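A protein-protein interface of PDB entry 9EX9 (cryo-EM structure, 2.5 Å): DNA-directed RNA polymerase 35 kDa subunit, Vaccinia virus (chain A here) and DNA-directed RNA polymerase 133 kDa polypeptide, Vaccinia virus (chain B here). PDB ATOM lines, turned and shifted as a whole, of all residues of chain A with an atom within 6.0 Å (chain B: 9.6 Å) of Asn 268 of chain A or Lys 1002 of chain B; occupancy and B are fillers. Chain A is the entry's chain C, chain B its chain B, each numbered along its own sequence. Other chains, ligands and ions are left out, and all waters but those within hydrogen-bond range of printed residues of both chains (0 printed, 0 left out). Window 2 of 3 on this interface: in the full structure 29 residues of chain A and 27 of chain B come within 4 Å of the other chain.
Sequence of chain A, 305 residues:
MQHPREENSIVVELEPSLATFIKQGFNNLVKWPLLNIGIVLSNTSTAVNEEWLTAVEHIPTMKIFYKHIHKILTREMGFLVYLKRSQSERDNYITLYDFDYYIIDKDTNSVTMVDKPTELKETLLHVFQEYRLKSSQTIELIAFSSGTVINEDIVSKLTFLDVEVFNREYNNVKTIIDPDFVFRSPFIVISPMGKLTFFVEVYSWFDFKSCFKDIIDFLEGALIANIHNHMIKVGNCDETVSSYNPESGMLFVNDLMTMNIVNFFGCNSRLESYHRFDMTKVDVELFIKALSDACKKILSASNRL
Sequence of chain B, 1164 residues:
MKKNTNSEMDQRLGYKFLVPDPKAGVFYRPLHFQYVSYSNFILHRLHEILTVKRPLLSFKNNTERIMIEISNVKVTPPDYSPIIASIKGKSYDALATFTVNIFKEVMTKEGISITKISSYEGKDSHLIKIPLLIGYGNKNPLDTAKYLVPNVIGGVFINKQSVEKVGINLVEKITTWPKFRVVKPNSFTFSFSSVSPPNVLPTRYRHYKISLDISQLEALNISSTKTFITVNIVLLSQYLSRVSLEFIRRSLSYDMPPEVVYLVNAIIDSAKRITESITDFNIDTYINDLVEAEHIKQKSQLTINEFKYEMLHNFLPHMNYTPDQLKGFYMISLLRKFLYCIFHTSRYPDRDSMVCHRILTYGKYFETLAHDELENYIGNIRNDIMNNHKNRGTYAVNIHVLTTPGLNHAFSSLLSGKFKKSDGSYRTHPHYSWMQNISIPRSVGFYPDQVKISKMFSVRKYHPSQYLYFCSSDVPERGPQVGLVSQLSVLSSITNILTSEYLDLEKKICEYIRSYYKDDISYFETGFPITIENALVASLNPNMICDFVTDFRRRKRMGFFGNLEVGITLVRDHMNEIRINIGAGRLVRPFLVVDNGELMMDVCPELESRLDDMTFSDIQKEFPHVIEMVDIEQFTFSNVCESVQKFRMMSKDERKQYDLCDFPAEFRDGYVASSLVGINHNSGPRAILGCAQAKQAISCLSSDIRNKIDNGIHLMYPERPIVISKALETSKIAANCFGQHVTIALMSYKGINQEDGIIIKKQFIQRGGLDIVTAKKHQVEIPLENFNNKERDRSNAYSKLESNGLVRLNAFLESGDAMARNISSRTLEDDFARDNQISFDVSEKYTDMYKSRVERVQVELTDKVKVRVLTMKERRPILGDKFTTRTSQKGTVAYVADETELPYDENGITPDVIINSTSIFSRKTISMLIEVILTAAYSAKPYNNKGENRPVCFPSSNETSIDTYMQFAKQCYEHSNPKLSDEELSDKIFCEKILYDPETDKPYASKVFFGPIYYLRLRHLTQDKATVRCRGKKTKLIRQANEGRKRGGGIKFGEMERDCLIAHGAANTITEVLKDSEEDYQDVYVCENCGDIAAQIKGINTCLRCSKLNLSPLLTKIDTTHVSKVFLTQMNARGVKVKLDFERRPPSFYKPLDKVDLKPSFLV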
ATOM      1  N   PRO A 192      15.409   7.289  -5.936  1.00  0.00           N
ATOM      2  CA  PRO A 192      15.079   6.113  -5.119  1.00  0.00           C
ATOM      3  C   PRO A 192      15.185   4.776  -5.837  1.00  0.00           C
ATOM      4  O   PRO A 192      15.933   3.905  -5.385  1.00  0.00           O
ATOM      5  CB  PRO A 192      13.638   6.397  -4.690  1.00  0.00           C
ATOM      6  CG  PRO A 192      13.556   7.862  -4.655  1.00  0.00           C
ATOM      7  CD  PRO A 192      14.405   8.353  -5.783  1.00  0.00           C
ATOM      8  N   MET A 193      14.450   4.576  -6.925  1.00  0.00           N
ATOM      9  CA  MET A 193      14.493   3.315  -7.667  1.00  0.00           C
ATOM     10  C   MET A 193      14.538   3.594  -9.162  1.00  0.00           C
ATOM     11  O   MET A 193      13.722   3.095  -9.937  1.00  0.00           O
ATOM     12  CB  MET A 193      13.303   2.425  -7.323  1.00  0.00           C
ATOM     13  CG  MET A 193      13.326   1.872  -5.909  1.00  0.00           C
ATOM     14  SD  MET A 193      14.563   0.590  -5.661  1.00  0.00           S
ATOM     15  CE  MET A 193      13.824  -0.778  -6.539  1.00  0.00           C
ATOM     16  N   VAL A 262      28.870  -1.822 -14.695  1.00  0.00           N
ATOM     17  CA  VAL A 262      28.666  -3.266 -14.760  1.00  0.00           C
ATOM     18  C   VAL A 262      27.239  -3.618 -14.368  1.00  0.00           C
ATOM     19  O   VAL A 262      26.650  -4.556 -14.915  1.00  0.00           O
ATOM     20  CB  VAL A 262      29.698  -4.007 -13.891  1.00  0.00           C
ATOM     21  CG1 VAL A 262      31.102  -3.658 -14.333  1.00  0.00           C
ATOM     22  CG2 VAL A 262      29.492  -3.701 -12.427  1.00  0.00           C
ATOM     23  N   ASN A 263      26.653  -2.882 -13.420  1.00  0.00           N
ATOM     24  CA  ASN A 263      25.250  -3.105 -13.098  1.00  0.00           C
ATOM     25  C   ASN A 263      24.354  -2.694 -14.256  1.00  0.00           C
ATOM     26  O   ASN A 263      23.302  -3.300 -14.479  1.00  0.00           O
ATOM     27  CB  ASN A 263      24.871  -2.338 -11.836  1.00  0.00           C
ATOM     28  CG  ASN A 263      25.643  -2.788 -10.630  1.00  0.00           C
ATOM     29  OD1 ASN A 263      26.692  -3.406 -10.752  1.00  0.00           O
ATOM     30  ND2 ASN A 263      25.133  -2.475  -9.452  1.00  0.00           N
ATOM     31  N   GLY A 266      24.019  -5.711 -16.459  1.00  0.00           N
ATOM     32  CA  GLY A 266      23.442  -6.950 -15.978  1.00  0.00           C
ATOM     33  C   GLY A 266      24.024  -7.543 -14.710  1.00  0.00           C
ATOM     34  O   GLY A 266      23.598  -8.633 -14.316  1.00  0.00           O
ATOM     35  N   CYS A 267      24.972  -6.877 -14.058  1.00  0.00           N
ATOM     36  CA  CYS A 267      25.515  -7.374 -12.801  1.00  0.00           C
ATOM     37  C   CYS A 267      24.738  -6.795 -11.616  1.00  0.00           C
ATOM     38  O   CYS A 267      23.911  -5.896 -11.762  1.00  0.00           O
ATOM     39  CB  CYS A 267      26.999  -7.032 -12.693  1.00  0.00           C
ATOM     40  SG  CYS A 267      27.855  -7.840 -11.336  1.00  0.00           S
ATOM     41  N   ASN A 268      25.022  -7.320 -10.426  1.00  0.00           N
ATOM     42  CA  ASN A 268      24.325  -6.948  -9.196  1.00  0.00           C
ATOM     43  C   ASN A 268      25.322  -6.713  -8.064  1.00  0.00           C
ATOM     44  O   ASN A 268      25.221  -7.295  -6.984  1.00  0.00           O
ATOM     45  CB  ASN A 268      23.315  -8.021  -8.813  1.00  0.00           C
ATOM     46  CG  ASN A 268      22.445  -7.611  -7.649  1.00  0.00           C
ATOM     47  OD1 ASN A 268      22.312  -6.428  -7.350  1.00  0.00           O
ATOM     48  ND2 ASN A 268      21.849  -8.588  -6.980  1.00  0.00           N
ATOM     49  N   SER A 269      26.309  -5.860  -8.301  1.00  0.00           N
ATOM     50  CA  SER A 269      27.468  -5.750  -7.429  1.00  0.00           C
ATOM     51  C   SER A 269      27.325  -4.633  -6.396  1.00  0.00           C
ATOM     52  O   SER A 269      26.571  -3.677  -6.572  1.00  0.00           O
ATOM     53  CB  SER A 269      28.718  -5.504  -8.263  1.00  0.00           C
ATOM     54  OG  SER A 269      28.519  -4.411  -9.138  1.00  0.00           O
ATOM     55  N   ARG A 270      28.074  -4.779  -5.304  1.00  0.00           N
ATOM     56  CA  ARG A 270      28.301  -3.751  -4.300  1.00  0.00           C
ATOM     57  C   ARG A 270      29.747  -3.274  -4.405  1.00  0.00           C
ATOM     58  O   ARG A 270      30.493  -3.690  -5.293  1.00  0.00           O
ATOM     59  CB  ARG A 270      27.984  -4.278  -2.900  1.00  0.00           C
ATOM     60  CG  ARG A 270      26.556  -4.077  -2.476  1.00  0.00           C
ATOM     61  CD  ARG A 270      26.382  -4.393  -1.009  1.00  0.00           C
ATOM     62  NE  ARG A 270      26.443  -3.190  -0.192  1.00  0.00           N
ATOM     63  CZ  ARG A 270      25.412  -2.388   0.036  1.00  0.00           C
ATOM     64  NH1 ARG A 270      24.221  -2.629  -0.482  1.00  0.00           N
ATOM     65  NH2 ARG A 270      25.581  -1.318   0.804  1.00  0.00           N
ATOM     66  N   HIS A 275      32.703 -10.718  -8.328  1.00  0.00           N
ATOM     67  CA  HIS A 275      31.577 -11.204  -9.112  1.00  0.00           C
ATOM     68  C   HIS A 275      32.080 -11.864 -10.385  1.00  0.00           C
ATOM     69  O   HIS A 275      33.112 -11.486 -10.942  1.00  0.00           O
ATOM     70  CB  HIS A 275      30.603 -10.072  -9.448  1.00  0.00           C
ATOM     71  CG  HIS A 275      29.942  -9.482  -8.246  1.00  0.00           C
ATOM     72  ND1 HIS A 275      28.828 -10.043  -7.662  1.00  0.00           N
ATOM     73  CD2 HIS A 275      30.252  -8.399  -7.499  1.00  0.00           C
ATOM     74  CE1 HIS A 275      28.476  -9.323  -6.613  1.00  0.00           C
ATOM     75  NE2 HIS A 275      29.324  -8.320  -6.492  1.00  0.00           N
ATOM     76  N   MET B 747      18.227   3.573  14.032  1.00  0.00           N
ATOM     77  CA  MET B 747      18.645   2.463  13.190  1.00  0.00           C
ATOM     78  C   MET B 747      20.106   2.171  13.471  1.00  0.00           C
ATOM     79  O   MET B 747      20.782   2.915  14.181  1.00  0.00           O
ATOM     80  CB  MET B 747      18.437   2.780  11.709  1.00  0.00           C
ATOM     81  CG  MET B 747      19.346   3.873  11.184  1.00  0.00           C
ATOM     82  SD  MET B 747      18.848   4.488   9.573  1.00  0.00           S
ATOM     83  CE  MET B 747      19.016   3.016   8.584  1.00  0.00           C
ATOM     84  N   LEU B 902      24.413   8.902   3.721  1.00  0.00           N
ATOM     85  CA  LEU B 902      23.369   8.647   4.695  1.00  0.00           C
ATOM     86  C   LEU B 902      22.086   8.201   4.005  1.00  0.00           C
ATOM     87  O   LEU B 902      21.820   8.604   2.871  1.00  0.00           O
ATOM     88  CB  LEU B 902      23.082   9.903   5.527  1.00  0.00           C
ATOM     89  CG  LEU B 902      24.201  10.390   6.445  1.00  0.00           C
ATOM     90  CD1 LEU B 902      23.872  11.749   7.000  1.00  0.00           C
ATOM     91  CD2 LEU B 902      24.425   9.411   7.570  1.00  0.00           C
ATOM     92  N   PRO B 903      21.276   7.371   4.657  1.00  0.00           N
ATOM     93  CA  PRO B 903      19.978   7.015   4.080  1.00  0.00           C
ATOM     94  C   PRO B 903      19.045   8.209   4.043  1.00  0.00           C
ATOM     95  O   PRO B 903      19.147   9.131   4.852  1.00  0.00           O
ATOM     96  CB  PRO B 903      19.458   5.929   5.025  1.00  0.00           C
ATOM     97  CG  PRO B 903      20.157   6.167   6.295  1.00  0.00           C
ATOM     98  CD  PRO B 903      21.503   6.700   5.945  1.00  0.00           C
ATOM     99  N   TYR B 904      18.123   8.187   3.088  1.00  0.00           N
ATOM    100  CA  TYR B 904      17.233   9.311   2.852  1.00  0.00           C
ATOM    101  C   TYR B 904      15.830   8.796   2.574  1.00  0.00           C
ATOM    102  O   TYR B 904      15.635   7.640   2.198  1.00  0.00           O
ATOM    103  CB  TYR B 904      17.726  10.171   1.684  1.00  0.00           C
ATOM    104  CG  TYR B 904      17.876   9.410   0.393  1.00  0.00           C
ATOM    105  CD1 TYR B 904      19.052   8.747   0.093  1.00  0.00           C
ATOM    106  CD2 TYR B 904      16.843   9.354  -0.525  1.00  0.00           C
ATOM    107  CE1 TYR B 904      19.194   8.053  -1.079  1.00  0.00           C
ATOM    108  CE2 TYR B 904      16.979   8.659  -1.702  1.00  0.00           C
ATOM    109  CZ  TYR B 904      18.156   8.012  -1.973  1.00  0.00           C
ATOM    110  OH  TYR B 904      18.298   7.319  -3.146  1.00  0.00           O
ATOM    111  N   ILE B 994      10.011   4.629   4.878  1.00  0.00           N
ATOM    112  CA  ILE B 994      10.892   3.767   4.106  1.00  0.00           C
ATOM    113  C   ILE B 994      12.109   4.590   3.715  1.00  0.00           C
ATOM    114  O   ILE B 994      11.977   5.635   3.070  1.00  0.00           O
ATOM    115  CB  ILE B 994      10.177   3.208   2.868  1.00  0.00           C
ATOM    116  CG1 ILE B 994       9.069   2.253   3.293  1.00  0.00           C
ATOM    117  CG2 ILE B 994      11.163   2.505   1.959  1.00  0.00           C
ATOM    118  CD1 ILE B 994       8.139   1.873   2.179  1.00  0.00           C
ATOM    119  N   LEU B 995      13.287   4.129   4.117  1.00  0.00           N
ATOM    120  CA  LEU B 995      14.546   4.786   3.809  1.00  0.00           C
ATOM    121  C   LEU B 995      15.294   3.981   2.757  1.00  0.00           C
ATOM    122  O   LEU B 995      15.117   2.768   2.645  1.00  0.00           O
ATOM    123  CB  LEU B 995      15.411   4.935   5.063  1.00  0.00           C
ATOM    124  CG  LEU B 995      14.806   5.729   6.223  1.00  0.00           C
ATOM    125  CD1 LEU B 995      15.779   5.800   7.366  1.00  0.00           C
ATOM    126  CD2 LEU B 995      14.416   7.119   5.791  1.00  0.00           C
ATOM    127  N   TYR B 996      16.132   4.669   1.986  1.00  0.00           N
ATOM    128  CA  TYR B 996      16.860   4.067   0.881  1.00  0.00           C
ATOM    129  C   TYR B 996      18.358   4.098   1.143  1.00  0.00           C
ATOM    130  O   TYR B 996      18.868   4.986   1.827  1.00  0.00           O
ATOM    131  CB  TYR B 996      16.560   4.784  -0.423  1.00  0.00           C
ATOM    132  CG  TYR B 996      15.129   4.653  -0.861  1.00  0.00           C
ATOM    133  CD1 TYR B 996      14.166   5.547  -0.425  1.00  0.00           C
ATOM    134  CD2 TYR B 996      14.737   3.634  -1.712  1.00  0.00           C
ATOM    135  CE1 TYR B 996      12.855   5.428  -0.823  1.00  0.00           C
ATOM    136  CE2 TYR B 996      13.429   3.508  -2.114  1.00  0.00           C
ATOM    137  CZ  TYR B 996      12.493   4.408  -1.670  1.00  0.00           C
ATOM    138  OH  TYR B 996      11.187   4.280  -2.074  1.00  0.00           O
ATOM    139  N   ASP B 997      19.051   3.114   0.592  1.00  0.00           N
ATOM    140  CA  ASP B 997      20.500   3.044   0.697  1.00  0.00           C
ATOM    141  C   ASP B 997      21.128   4.011  -0.300  1.00  0.00           C
ATOM    142  O   ASP B 997      20.885   3.882  -1.504  1.00  0.00           O
ATOM    143  CB  ASP B 997      20.966   1.622   0.422  1.00  0.00           C
ATOM    144  CG  ASP B 997      22.429   1.406   0.745  1.00  0.00           C
ATOM    145  OD1 ASP B 997      23.183   2.391   0.819  1.00  0.00           O
ATOM    146  OD2 ASP B 997      22.828   0.238   0.918  1.00  0.00           O
ATOM    147  N   PRO B 998      21.929   4.984   0.142  1.00  0.00           N
ATOM    148  CA  PRO B 998      22.487   5.951  -0.813  1.00  0.00           C
ATOM    149  C   PRO B 998      23.383   5.325  -1.858  1.00  0.00           C
ATOM    150  O   PRO B 998      23.516   5.874  -2.958  1.00  0.00           O
ATOM    151  CB  PRO B 998      23.273   6.908   0.087  1.00  0.00           C
ATOM    152  CG  PRO B 998      23.614   6.105   1.271  1.00  0.00           C
ATOM    153  CD  PRO B 998      22.439   5.218   1.502  1.00  0.00           C
ATOM    154  N   GLU B 999      24.020   4.201  -1.540  1.00  0.00           N
ATOM    155  CA  GLU B 999      24.997   3.615  -2.448  1.00  0.00           C
ATOM    156  C   GLU B 999      24.325   2.938  -3.636  1.00  0.00           C
ATOM    157  O   GLU B 999      24.799   3.055  -4.770  1.00  0.00           O
ATOM    158  CB  GLU B 999      25.869   2.623  -1.687  1.00  0.00           C
ATOM    159  CG  GLU B 999      26.841   1.867  -2.549  1.00  0.00           C
ATOM    160  CD  GLU B 999      27.822   1.059  -1.734  1.00  0.00           C
ATOM    161  OE1 GLU B 999      28.224   1.525  -0.650  1.00  0.00           O
ATOM    162  OE2 GLU B 999      28.184  -0.050  -2.168  1.00  0.00           O
ATOM    163  N   THR B1000      23.225   2.227  -3.401  1.00  0.00           N
ATOM    164  CA  THR B1000      22.552   1.477  -4.449  1.00  0.00           C
ATOM    165  C   THR B1000      21.178   2.018  -4.801  1.00  0.00           C
ATOM    166  O   THR B1000      20.625   1.617  -5.829  1.00  0.00           O
ATOM    167  CB  THR B1000      22.406   0.008  -4.036  1.00  0.00           C
ATOM    168  OG1 THR B1000      21.533  -0.088  -2.909  1.00  0.00           O
ATOM    169  CG2 THR B1000      23.751  -0.575  -3.671  1.00  0.00           C
ATOM    170  N   ASP B1001      20.615   2.913  -3.992  1.00  0.00           N
ATOM    171  CA  ASP B1001      19.264   3.431  -4.204  1.00  0.00           C
ATOM    172  C   ASP B1001      18.239   2.298  -4.194  1.00  0.00           C
ATOM    173  O   ASP B1001      17.515   2.070  -5.159  1.00  0.00           O
ATOM    174  CB  ASP B1001      19.179   4.226  -5.510  1.00  0.00           C
ATOM    175  CG  ASP B1001      20.000   5.492  -5.476  1.00  0.00           C
ATOM    176  OD1 ASP B1001      20.606   5.779  -4.429  1.00  0.00           O
ATOM    177  OD2 ASP B1001      20.042   6.204  -6.497  1.00  0.00           O
ATOM    178  N   LYS B1002      18.202   1.579  -3.080  1.00  0.00           N
ATOM    179  CA  LYS B1002      17.239   0.513  -2.873  1.00  0.00           C
ATOM    180  C   LYS B1002      16.731   0.568  -1.442  1.00  0.00           C
ATOM    181  O   LYS B1002      17.473   0.964  -0.537  1.00  0.00           O
ATOM    182  CB  LYS B1002      17.855  -0.864  -3.151  1.00  0.00           C
ATOM    183  CG  LYS B1002      18.215  -1.092  -4.601  1.00  0.00           C
ATOM    184  CD  LYS B1002      18.935  -2.407  -4.785  1.00  0.00           C
ATOM    185  CE  LYS B1002      19.293  -2.645  -6.233  1.00  0.00           C
ATOM    186  NZ  LYS B1002      20.034  -3.920  -6.406  1.00  0.00           N
ATOM    187  N   PRO B1003      15.488   0.162  -1.201  1.00  0.00           N
ATOM    188  CA  PRO B1003      14.923   0.284   0.143  1.00  0.00           C
ATOM    189  C   PRO B1003      15.545  -0.704   1.111  1.00  0.00           C
ATOM    190  O   PRO B1003      16.133  -1.714   0.725  1.00  0.00           O
ATOM    191  CB  PRO B1003      13.435  -0.019  -0.061  1.00  0.00           C
ATOM    192  CG  PRO B1003      13.231  -0.128  -1.533  1.00  0.00           C
ATOM    193  CD  PRO B1003      14.540  -0.485  -2.118  1.00  0.00           C
ATOM    194  N   TYR B1004      15.406  -0.397   2.394  1.00  0.00           N
ATOM    195  CA  TYR B1004      15.775  -1.345   3.428  1.00  0.00           C
ATOM    196  C   TYR B1004      14.618  -2.301   3.700  1.00  0.00           C
ATOM    197  O   TYR B1004      13.519  -2.162   3.160  1.00  0.00           O
ATOM    198  CB  TYR B1004      16.182  -0.618   4.705  1.00  0.00           C
ATOM    199  CG  TYR B1004      17.534   0.044   4.626  1.00  0.00           C
ATOM    200  CD1 TYR B1004      18.694  -0.699   4.740  1.00  0.00           C
ATOM    201  CD2 TYR B1004      17.650   1.409   4.446  1.00  0.00           C
ATOM    202  CE1 TYR B1004      19.926  -0.104   4.675  1.00  0.00           C
ATOM    203  CE2 TYR B1004      18.880   2.010   4.379  1.00  0.00           C
ATOM    204  CZ  TYR B1004      20.013   1.248   4.492  1.00  0.00           C
ATOM    205  OH  TYR B1004      21.250   1.840   4.428  1.00  0.00           O
ATOM    206  N   ALA B1005      14.880  -3.287   4.557  1.00  0.00           N
ATOM    207  CA  ALA B1005      13.924  -4.371   4.757  1.00  0.00           C
ATOM    208  C   ALA B1005      12.616  -3.868   5.354  1.00  0.00           C
ATOM    209  O   ALA B1005      11.531  -4.243   4.899  1.00  0.00           O
ATOM    210  CB  ALA B1005      14.541  -5.444   5.650  1.00  0.00           C
ATOM    211  N   SER B1006      12.696  -3.020   6.377  1.00  0.00           N
ATOM    212  CA  SER B1006      11.519  -2.585   7.114  1.00  0.00           C
ATOM    213  C   SER B1006      11.584  -1.084   7.344  1.00  0.00           C
ATOM    214  O   SER B1006      12.595  -0.434   7.075  1.00  0.00           O
ATOM    215  CB  SER B1006      11.398  -3.328   8.447  1.00  0.00           C
ATOM    216  OG  SER B1006      12.633  -3.334   9.137  1.00  0.00           O
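Of chain B, only Lys 1002 (3.5 Å) comes within 4 Å of Asn 268 of chain A. No residue of chain B comes within 4 Å of Cys 267 of chain A. No residue of chain B comes within 4 Å of Ser 269 of chain A. Printed residues of chain A within 4 Å of Asp 997 of chain B: Arg 270. Of the printed residues of chain B, Met 193 of chain A touches Asp 1001, Lys 1002 and Pro 1003. Val 262 of chain A touches none of the printed residues of chain B. Ala 1005 of chain B touches none of the printed residues of chain A. The nearest printed residue of chain A that does not touch Thr 1000 of chain B is Ser 269 of chain A (5.1 Å).
Among the printed residues, merely in contact across the chains: Asn 268 of chain A with Lys 1002 of chain B (3.5 Å), Met 193 of chain A with Pro 1003 of chain B (3.7 Å), Pro 192 of chain A with Tyr 996 of chain B (3.8 Å), Arg 270 of chain A with Thr 1000 of chain B (3.8 Å), Met 193 of chain A with Lys 1002 of chain B (3.9 Å), Pro 192 of chain A with Tyr 904 of chain B (3.96 Å) and Pro 192 of chain A with Lys 1002 of chain B (3.98 Å).
The backbone carbonyl oxygen (O) of Tyr 904 of chain B sits at hydrogen-bond distance from the backbone NH (N) of Tyr 996 of chain B. The side-chain carboxylate of Asp 997 of chain B is in hydrogen-bond range of the backbone NH of Glu 999 of chain B, 3.1 Å away. OH of Tyr 904 of chain B is in hydrogen-bond range of OD1 of Asp 1001 of chain B, 3.1 Å away. N of Asp 997 of chain B lies within hydrogen-bond range of O of Lys 1002 of chain B.
Of the 10 printed residues of chain A, 4 touch a printed residue of chain B. Hydrophobic or aromatic side chains of chain A within 4 Å of the printed part of chain B: Pro 192 and Met 193. Among the printed residues, Asp or Glu carboxylates within 4 Å of a Lys or Arg side-chain nitrogen of the other chain: Arg 270 of chain A with Asp 997 of chain B (3.2 Å).
The side-chain carboxylate of Asp 997 of chain B lies within salt-bridge range of the guanidinium group of Arg 270 of chain A (3.2 Å). O of Asp 1001 of chain B sits close to O of Pro 192 of chain A. The side-chain sulfur (SD) of Met 193 of chain A lies close to the backbone carbonyl oxygen (O) of Asp 1001 of chain B (3.3 Å).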
